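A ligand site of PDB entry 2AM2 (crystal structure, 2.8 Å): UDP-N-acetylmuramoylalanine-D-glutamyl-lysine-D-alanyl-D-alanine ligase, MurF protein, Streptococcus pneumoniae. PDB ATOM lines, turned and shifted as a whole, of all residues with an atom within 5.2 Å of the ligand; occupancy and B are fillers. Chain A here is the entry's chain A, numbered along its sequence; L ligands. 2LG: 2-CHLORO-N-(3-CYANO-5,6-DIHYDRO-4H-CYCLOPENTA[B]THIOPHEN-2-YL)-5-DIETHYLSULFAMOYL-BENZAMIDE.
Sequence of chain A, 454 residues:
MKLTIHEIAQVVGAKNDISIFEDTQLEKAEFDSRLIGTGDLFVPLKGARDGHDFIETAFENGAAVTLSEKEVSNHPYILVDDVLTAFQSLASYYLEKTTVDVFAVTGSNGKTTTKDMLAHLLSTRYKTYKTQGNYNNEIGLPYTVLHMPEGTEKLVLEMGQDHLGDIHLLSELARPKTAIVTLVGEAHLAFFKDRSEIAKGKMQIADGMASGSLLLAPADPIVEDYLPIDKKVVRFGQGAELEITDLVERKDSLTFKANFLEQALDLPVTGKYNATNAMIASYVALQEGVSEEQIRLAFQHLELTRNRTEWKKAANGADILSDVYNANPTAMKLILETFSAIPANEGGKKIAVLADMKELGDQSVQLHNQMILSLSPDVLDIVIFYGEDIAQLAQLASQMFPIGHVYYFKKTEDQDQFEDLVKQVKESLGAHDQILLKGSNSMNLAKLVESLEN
A sulfur (S5) of the ligand sits close to the guanidinium group of Arg 34, 3.0 Å away.
The side-chain amide nitrogen of Asn 326 is in hydrogen-bond range of an oxygen (O24) of the ligand (3.1 Å).
N11 of the ligand lies within hydrogen-bond range of N of Arg 49.
The backbone NH of Ala 48 sits at hydrogen-bond distance from a nitrogen (N11) of the ligand, 3.1 Å away.
The side-chain hydroxyl (OG1) of Thr 330 is in hydrogen-bond range of a nitrogen (N10) of the ligand, 3.3 Å away.
The backbone NH (N) of Ile 139 sits close to the side-chain amide oxygen (OD1) of Asn 137, 3.5 Å away.
The side-chain amide oxygen (OD1) of Asn 137 lies within hydrogen-bond range of the backbone NH (N) of Gly 140 (2.8 Å).
The side-chain carboxylate (OD2) of Asp 32 lies within salt-bridge range of the guanidinium group (NH2) of Arg 34, at 3.1 Å.
OD1 of Asn 326 sits close to OD1 of Asn 134 (2.9 Å).
The side-chain hydroxyl (OG1) of Thr 330 lies within hydrogen-bond range of the backbone NH (N) of Ala 48, 2.5 Å away.
N of Thr 330 lies within hydrogen-bond range of OD1 of Asn 328 (3.1 Å).
N of Ala 331 sits at hydrogen-bond distance from OD1 of Asn 328, 2.8 Å away.
The side-chain carboxylate (OD1) of Asp 32 lies close to a sulfur (S5) of the ligand (3.6 Å).
Merely in contact with the ligand: Asn 137, Tyr 135, Asn 134, Leu 367, Asn 328, Phe 31, Ala 331 and Gly 47.
Hydrophobic or aromatic side chains that line the ligand: Phe 31, Ala 48, Tyr 135 and Leu 367.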
ATOM      1  N   PHE A  31      -4.824 -16.279  -2.001  1.00  0.00           N
ATOM      2  CA  PHE A  31      -3.466 -16.800  -2.091  1.00  0.00           C
ATOM      3  C   PHE A  31      -3.426 -18.061  -1.235  1.00  0.00           C
ATOM      4  O   PHE A  31      -2.480 -18.843  -1.271  1.00  0.00           O
ATOM      5  CB  PHE A  31      -2.459 -15.768  -1.592  1.00  0.00           C
ATOM      6  CG  PHE A  31      -2.801 -15.142  -0.265  1.00  0.00           C
ATOM      7  CD1 PHE A  31      -2.985 -13.777  -0.153  1.00  0.00           C
ATOM      8  CD2 PHE A  31      -2.924 -15.918   0.871  1.00  0.00           C
ATOM      9  CE1 PHE A  31      -3.284 -13.206   1.059  1.00  0.00           C
ATOM     10  CE2 PHE A  31      -3.223 -15.347   2.082  1.00  0.00           C
ATOM     11  CZ  PHE A  31      -3.402 -14.006   2.180  1.00  0.00           C
ATOM     12  N   ASP A  32      -4.497 -18.212  -0.467  1.00  0.00           N
ATOM     13  CA  ASP A  32      -4.701 -19.335   0.437  1.00  0.00           C
ATOM     14  C   ASP A  32      -5.724 -20.264  -0.237  1.00  0.00           C
ATOM     15  O   ASP A  32      -6.925 -20.129  -0.053  1.00  0.00           O
ATOM     16  CB  ASP A  32      -5.220 -18.782   1.782  1.00  0.00           C
ATOM     17  CG  ASP A  32      -5.690 -19.865   2.737  1.00  0.00           C
ATOM     18  OD1 ASP A  32      -5.202 -21.016   2.640  1.00  0.00           O
ATOM     19  OD2 ASP A  32      -6.531 -19.558   3.617  1.00  0.00           O
ATOM     20  N   ARG A  34      -7.028 -22.699   0.308  1.00  0.00           N
ATOM     21  CA  ARG A  34      -8.077 -23.137   1.221  1.00  0.00           C
ATOM     22  C   ARG A  34      -9.204 -22.108   1.343  1.00  0.00           C
ATOM     23  O   ARG A  34     -10.207 -22.361   2.011  1.00  0.00           O
ATOM     24  CB  ARG A  34      -7.431 -23.420   2.583  1.00  0.00           C
ATOM     25  CG  ARG A  34      -8.370 -23.901   3.674  1.00  0.00           C
ATOM     26  CD  ARG A  34      -7.637 -23.863   4.980  1.00  0.00           C
ATOM     27  NE  ARG A  34      -6.601 -22.826   4.927  1.00  0.00           N
ATOM     28  CZ  ARG A  34      -6.061 -22.241   5.989  1.00  0.00           C
ATOM     29  NH1 ARG A  34      -6.430 -22.579   7.218  1.00  0.00           N
ATOM     30  NH2 ARG A  34      -5.125 -21.311   5.816  1.00  0.00           N
ATOM     31  N   LEU A  45       1.579 -17.742  -4.001  1.00  0.00           N
ATOM     32  CA  LEU A  45       2.672 -16.968  -3.422  1.00  0.00           C
ATOM     33  C   LEU A  45       3.720 -17.840  -2.723  1.00  0.00           C
ATOM     34  O   LEU A  45       3.496 -19.029  -2.476  1.00  0.00           O
ATOM     35  CB  LEU A  45       2.100 -15.959  -2.416  1.00  0.00           C
ATOM     36  CG  LEU A  45       1.157 -14.884  -2.956  1.00  0.00           C
ATOM     37  CD1 LEU A  45       0.430 -14.217  -1.800  1.00  0.00           C
ATOM     38  CD2 LEU A  45       1.942 -13.873  -3.769  1.00  0.00           C
ATOM     39  N   GLY A  47       4.936 -18.933   0.286  1.00  0.00           N
ATOM     40  CA  GLY A  47       4.601 -18.990   1.702  1.00  0.00           C
ATOM     41  C   GLY A  47       5.478 -19.962   2.451  1.00  0.00           C
ATOM     42  O   GLY A  47       6.634 -20.136   2.095  1.00  0.00           O
ATOM     43  N   ALA A  48       4.951 -20.587   3.505  1.00  0.00           N
ATOM     44  CA  ALA A  48       5.730 -21.571   4.267  1.00  0.00           C
ATOM     45  C   ALA A  48       6.133 -22.623   3.246  1.00  0.00           C
ATOM     46  O   ALA A  48       7.265 -23.101   3.230  1.00  0.00           O
ATOM     47  CB  ALA A  48       4.861 -22.170   5.342  1.00  0.00           C
ATOM     48  N   ARG A  49       5.162 -22.982   2.401  1.00  0.00           N
ATOM     49  CA  ARG A  49       5.359 -23.918   1.298  1.00  0.00           C
ATOM     50  C   ARG A  49       4.962 -23.076   0.085  1.00  0.00           C
ATOM     51  O   ARG A  49       4.099 -22.201   0.203  1.00  0.00           O
ATOM     52  CB  ARG A  49       4.417 -25.119   1.432  1.00  0.00           C
ATOM     53  CG  ARG A  49       4.772 -26.034   2.572  1.00  0.00           C
ATOM     54  CD  ARG A  49       4.032 -27.352   2.482  1.00  0.00           C
ATOM     55  NE  ARG A  49       4.966 -28.483   2.546  1.00  0.00           N
ATOM     56  CZ  ARG A  49       5.681 -28.920   1.518  1.00  0.00           C
ATOM     57  NH1 ARG A  49       5.606 -28.332   0.334  1.00  0.00           N
ATOM     58  NH2 ARG A  49       6.502 -29.946   1.687  1.00  0.00           N
ATOM     59  N   PHE A  54      -0.292 -25.682  -4.718  1.00  0.00           N
ATOM     60  CA  PHE A  54      -1.696 -25.793  -4.351  1.00  0.00           C
ATOM     61  C   PHE A  54      -2.641 -25.366  -5.443  1.00  0.00           C
ATOM     62  O   PHE A  54      -3.850 -25.213  -5.222  1.00  0.00           O
ATOM     63  CB  PHE A  54      -1.971 -24.963  -3.102  1.00  0.00           C
ATOM     64  CG  PHE A  54      -1.213 -25.415  -1.880  1.00  0.00           C
ATOM     65  CD1 PHE A  54       0.156 -25.576  -1.909  1.00  0.00           C
ATOM     66  CD2 PHE A  54      -1.885 -25.646  -0.695  1.00  0.00           C
ATOM     67  CE1 PHE A  54       0.849 -25.965  -0.785  1.00  0.00           C
ATOM     68  CE2 PHE A  54      -1.192 -26.028   0.445  1.00  0.00           C
ATOM     69  CZ  PHE A  54       0.174 -26.191   0.392  1.00  0.00           C
ATOM     70  N   ASN A 134      -4.239  -7.279  10.068  1.00  0.00           N
ATOM     71  CA  ASN A 134      -2.877  -6.788   9.933  1.00  0.00           C
ATOM     72  C   ASN A 134      -2.379  -7.042   8.519  1.00  0.00           C
ATOM     73  O   ASN A 134      -1.189  -7.222   8.267  1.00  0.00           O
ATOM     74  CB  ASN A 134      -1.943  -7.460  10.954  1.00  0.00           C
ATOM     75  CG  ASN A 134      -1.799  -8.949  10.729  1.00  0.00           C
ATOM     76  OD1 ASN A 134      -2.786  -9.680  10.695  1.00  0.00           O
ATOM     77  ND2 ASN A 134      -0.556  -9.413  10.590  1.00  0.00           N
ATOM     78  N   TYR A 135      -3.333  -7.062   7.591  1.00  0.00           N
ATOM     79  CA  TYR A 135      -3.039  -7.254   6.184  1.00  0.00           C
ATOM     80  C   TYR A 135      -2.491  -5.919   5.683  1.00  0.00           C
ATOM     81  O   TYR A 135      -3.021  -5.356   4.730  1.00  0.00           O
ATOM     82  CB  TYR A 135      -4.330  -7.600   5.428  1.00  0.00           C
ATOM     83  CG  TYR A 135      -4.572  -9.076   5.159  1.00  0.00           C
ATOM     84  CD1 TYR A 135      -4.310  -9.619   3.904  1.00  0.00           C
ATOM     85  CD2 TYR A 135      -5.109  -9.905   6.131  1.00  0.00           C
ATOM     86  CE1 TYR A 135      -4.562 -10.940   3.639  1.00  0.00           C
ATOM     87  CE2 TYR A 135      -5.366 -11.234   5.864  1.00  0.00           C
ATOM     88  CZ  TYR A 135      -5.091 -11.748   4.607  1.00  0.00           C
ATOM     89  OH  TYR A 135      -5.330 -13.072   4.325  1.00  0.00           O
ATOM     90  N   ASN A 136      -1.444  -5.423   6.329  1.00  0.00           N
ATOM     91  CA  ASN A 136      -0.864  -4.147   5.952  1.00  0.00           C
ATOM     92  C   ASN A 136       0.534  -4.230   5.376  1.00  0.00           C
ATOM     93  O   ASN A 136       1.299  -3.263   5.457  1.00  0.00           O
ATOM     94  CB  ASN A 136      -0.862  -3.178   7.149  1.00  0.00           C
ATOM     95  CG  ASN A 136       0.161  -3.551   8.221  1.00  0.00           C
ATOM     96  OD1 ASN A 136       0.973  -4.452   8.058  1.00  0.00           O
ATOM     97  ND2 ASN A 136       0.123  -2.837   9.329  1.00  0.00           N
ATOM     98  N   ASN A 137       0.869  -5.369   4.780  1.00  0.00           N
ATOM     99  CA  ASN A 137       2.197  -5.565   4.201  1.00  0.00           C
ATOM    100  C   ASN A 137       2.101  -5.719   2.682  1.00  0.00           C
ATOM    101  O   ASN A 137       1.023  -5.589   2.101  1.00  0.00           O
ATOM    102  CB  ASN A 137       2.840  -6.805   4.798  1.00  0.00           C
ATOM    103  CG  ASN A 137       2.163  -8.062   4.341  1.00  0.00           C
ATOM    104  OD1 ASN A 137       0.935  -8.136   4.292  1.00  0.00           O
ATOM    105  ND2 ASN A 137       2.952  -9.064   3.990  1.00  0.00           N
ATOM    106  N   ILE A 139       1.660  -8.015   0.888  1.00  0.00           N
ATOM    107  CA  ILE A 139       0.709  -9.028   0.405  1.00  0.00           C
ATOM    108  C   ILE A 139      -0.690  -8.593   0.816  1.00  0.00           C
ATOM    109  O   ILE A 139      -1.634  -8.683   0.049  1.00  0.00           O
ATOM    110  CB  ILE A 139       0.944 -10.445   1.017  1.00  0.00           C
ATOM    111  CG1 ILE A 139       2.126 -11.155   0.362  1.00  0.00           C
ATOM    112  CG2 ILE A 139      -0.313 -11.279   0.826  1.00  0.00           C
ATOM    113  CD1 ILE A 139       3.482 -10.722   0.860  1.00  0.00           C
ATOM    114  N   GLY A 140      -0.792  -8.099   2.040  1.00  0.00           N
ATOM    115  CA  GLY A 140      -2.058  -7.668   2.572  1.00  0.00           C
ATOM    116  C   GLY A 140      -2.667  -6.460   1.886  1.00  0.00           C
ATOM    117  O   GLY A 140      -3.883  -6.393   1.720  1.00  0.00           O
ATOM    118  N   ASN A 326      -3.633 -14.866  12.904  1.00  0.00           N
ATOM    119  CA  ASN A 326      -2.777 -15.329  11.815  1.00  0.00           C
ATOM    120  C   ASN A 326      -2.216 -16.715  12.101  1.00  0.00           C
ATOM    121  O   ASN A 326      -1.002 -16.929  12.023  1.00  0.00           O
ATOM    122  CB  ASN A 326      -1.625 -14.360  11.569  1.00  0.00           C
ATOM    123  CG  ASN A 326      -1.991 -13.220  10.649  1.00  0.00           C
ATOM    124  OD1 ASN A 326      -3.026 -12.576  10.841  1.00  0.00           O
ATOM    125  ND2 ASN A 326      -1.158 -12.973   9.657  1.00  0.00           N
ATOM    126  N   ASN A 328      -1.292 -19.618  10.831  1.00  0.00           N
ATOM    127  CA  ASN A 328      -0.975 -20.340   9.626  1.00  0.00           C
ATOM    128  C   ASN A 328       0.533 -20.407   9.519  1.00  0.00           C
ATOM    129  O   ASN A 328       1.227 -19.568  10.075  1.00  0.00           O
ATOM    130  CB  ASN A 328      -1.547 -19.623   8.391  1.00  0.00           C
ATOM    131  CG  ASN A 328      -0.784 -18.359   8.054  1.00  0.00           C
ATOM    132  OD1 ASN A 328       0.277 -18.395   7.425  1.00  0.00           O
ATOM    133  ND2 ASN A 328      -1.304 -17.225   8.471  1.00  0.00           N
ATOM    134  N   PRO A 329       1.049 -21.419   8.802  1.00  0.00           N
ATOM    135  CA  PRO A 329       2.462 -21.684   8.572  1.00  0.00           C
ATOM    136  C   PRO A 329       3.280 -20.458   8.232  1.00  0.00           C
ATOM    137  O   PRO A 329       4.149 -20.052   8.994  1.00  0.00           O
ATOM    138  CB  PRO A 329       2.428 -22.706   7.451  1.00  0.00           C
ATOM    139  CG  PRO A 329       1.244 -23.514   7.807  1.00  0.00           C
ATOM    140  CD  PRO A 329       0.234 -22.439   8.128  1.00  0.00           C
ATOM    141  N   THR A 330       2.982 -19.853   7.083  1.00  0.00           N
ATOM    142  CA  THR A 330       3.713 -18.662   6.646  1.00  0.00           C
ATOM    143  C   THR A 330       3.779 -17.589   7.737  1.00  0.00           C
ATOM    144  O   THR A 330       4.826 -16.984   7.956  1.00  0.00           O
ATOM    145  CB  THR A 330       3.084 -18.069   5.375  1.00  0.00           C
ATOM    146  OG1 THR A 330       3.195 -18.988   4.285  1.00  0.00           O
ATOM    147  CG2 THR A 330       3.790 -16.783   5.009  1.00  0.00           C
ATOM    148  N   ALA A 331       2.661 -17.343   8.415  1.00  0.00           N
ATOM    149  CA  ALA A 331       2.619 -16.349   9.475  1.00  0.00           C
ATOM    150  C   ALA A 331       3.668 -16.679  10.514  1.00  0.00           C
ATOM    151  O   ALA A 331       4.506 -15.841  10.845  1.00  0.00           O
ATOM    152  CB  ALA A 331       1.248 -16.320  10.120  1.00  0.00           C
ATOM    153  N   LEU A 334       7.242 -16.433   9.435  1.00  0.00           N
ATOM    154  CA  LEU A 334       7.757 -15.066   9.424  1.00  0.00           C
ATOM    155  C   LEU A 334       7.928 -14.614  10.866  1.00  0.00           C
ATOM    156  O   LEU A 334       9.015 -14.224  11.287  1.00  0.00           O
ATOM    157  CB  LEU A 334       6.807 -14.116   8.700  1.00  0.00           C
ATOM    158  CG  LEU A 334       6.671 -14.307   7.186  1.00  0.00           C
ATOM    159  CD1 LEU A 334       5.972 -13.097   6.603  1.00  0.00           C
ATOM    160  CD2 LEU A 334       8.044 -14.480   6.557  1.00  0.00           C
ATOM    161  N   LEU A 360      -5.215 -26.453   9.576  1.00  0.00           N
ATOM    162  CA  LEU A 360      -4.315 -26.505   8.435  1.00  0.00           C
ATOM    163  C   LEU A 360      -4.814 -27.595   7.501  1.00  0.00           C
ATOM    164  O   LEU A 360      -4.406 -27.683   6.348  1.00  0.00           O
ATOM    165  CB  LEU A 360      -2.885 -26.806   8.878  1.00  0.00           C
ATOM    166  CG  LEU A 360      -2.303 -25.761   9.819  1.00  0.00           C
ATOM    167  CD1 LEU A 360      -0.786 -25.855   9.813  1.00  0.00           C
ATOM    168  CD2 LEU A 360      -2.756 -24.377   9.379  1.00  0.00           C
ATOM    169  N   LEU A 367       2.626 -29.782   7.691  1.00  0.00           N
ATOM    170  CA  LEU A 367       2.768 -28.335   7.752  1.00  0.00           C
ATOM    171  C   LEU A 367       3.559 -27.837   8.944  1.00  0.00           C
ATOM    172  O   LEU A 367       4.413 -26.962   8.805  1.00  0.00           O
ATOM    173  CB  LEU A 367       1.390 -27.689   7.727  1.00  0.00           C
ATOM    174  CG  LEU A 367       0.688 -27.740   6.356  1.00  0.00           C
ATOM    175  CD1 LEU A 367      -0.725 -27.209   6.493  1.00  0.00           C
ATOM    176  CD2 LEU A 367       1.505 -26.954   5.317  1.00  0.00           C
HETATM  177  C4  2LG L   1      -0.841 -24.377   4.275  1.00  0.00           C
HETATM  178  C6  2LG L   1      -2.975 -23.839   5.150  1.00  0.00           C
HETATM  179  C7  2LG L   1      -0.685 -20.533   4.160  1.00  0.00           C
HETATM  180  C8  2LG L   1       1.193 -21.926   3.415  1.00  0.00           C
HETATM  181  C13 2LG L   1      -0.044 -16.911   3.622  1.00  0.00           C
HETATM  182  C15 2LG L   1       0.037 -16.017   4.694  1.00  0.00           C
HETATM  183  C17 2LG L   1       0.719 -14.793   4.575  1.00  0.00           C
HETATM  184  C21 2LG L   1       1.338 -14.437   3.345  1.00  0.00           C
HETATM  185  C26 2LG L   1      -0.705 -11.754   4.911  1.00  0.00           C
HETATM  186  C28 2LG L   1      -1.959 -12.119   5.719  1.00  0.00           C
HETATM  187  C1  2LG L   1      -1.012 -22.891   4.330  1.00  0.00           C
HETATM  188  C2  2LG L   1      -2.215 -22.589   4.818  1.00  0.00           C
HETATM  189  C3  2LG L   1      -0.152 -21.745   3.956  1.00  0.00           C
HETATM  190  S5  2LG L   1      -2.291 -20.826   4.826  1.00  0.00           S
HETATM  191  C9  2LG L   1      -2.266 -24.942   4.344  1.00  0.00           C
HETATM  192  N10 2LG L   1      -0.107 -19.317   3.893  1.00  0.00           N
HETATM  193  N11 2LG L   1       2.267 -22.071   2.983  1.00  0.00           N
HETATM  194  C12 2LG L   1      -0.781 -18.161   3.864  1.00  0.00           C
HETATM  195  O14 2LG L   1      -1.988 -18.111   4.087  1.00  0.00           O
HETATM  196  C16 2LG L   1       0.576 -16.582   2.353  1.00  0.00           C
HETATM  197  C18 2LG L   1       1.259 -15.333   2.235  1.00  0.00           C
HETATM  198 CL19 2LG L   1       0.511 -17.663   0.973  1.00  0.00          CL
HETATM  199  S20 2LG L   1       0.776 -13.725   6.057  1.00  0.00           S
HETATM  200  N22 2LG L   1       0.618 -12.013   5.649  1.00  0.00           N
HETATM  201  O23 2LG L   1       2.052 -13.892   6.683  1.00  0.00           O
HETATM  202  O24 2LG L   1      -0.238 -14.127   6.978  1.00  0.00           O
HETATM  203  C25 2LG L   1       0.682 -11.259   6.959  1.00  0.00           C
HETATM  204  C27 2LG L   1       0.575  -9.732   6.790  1.00  0.00           C
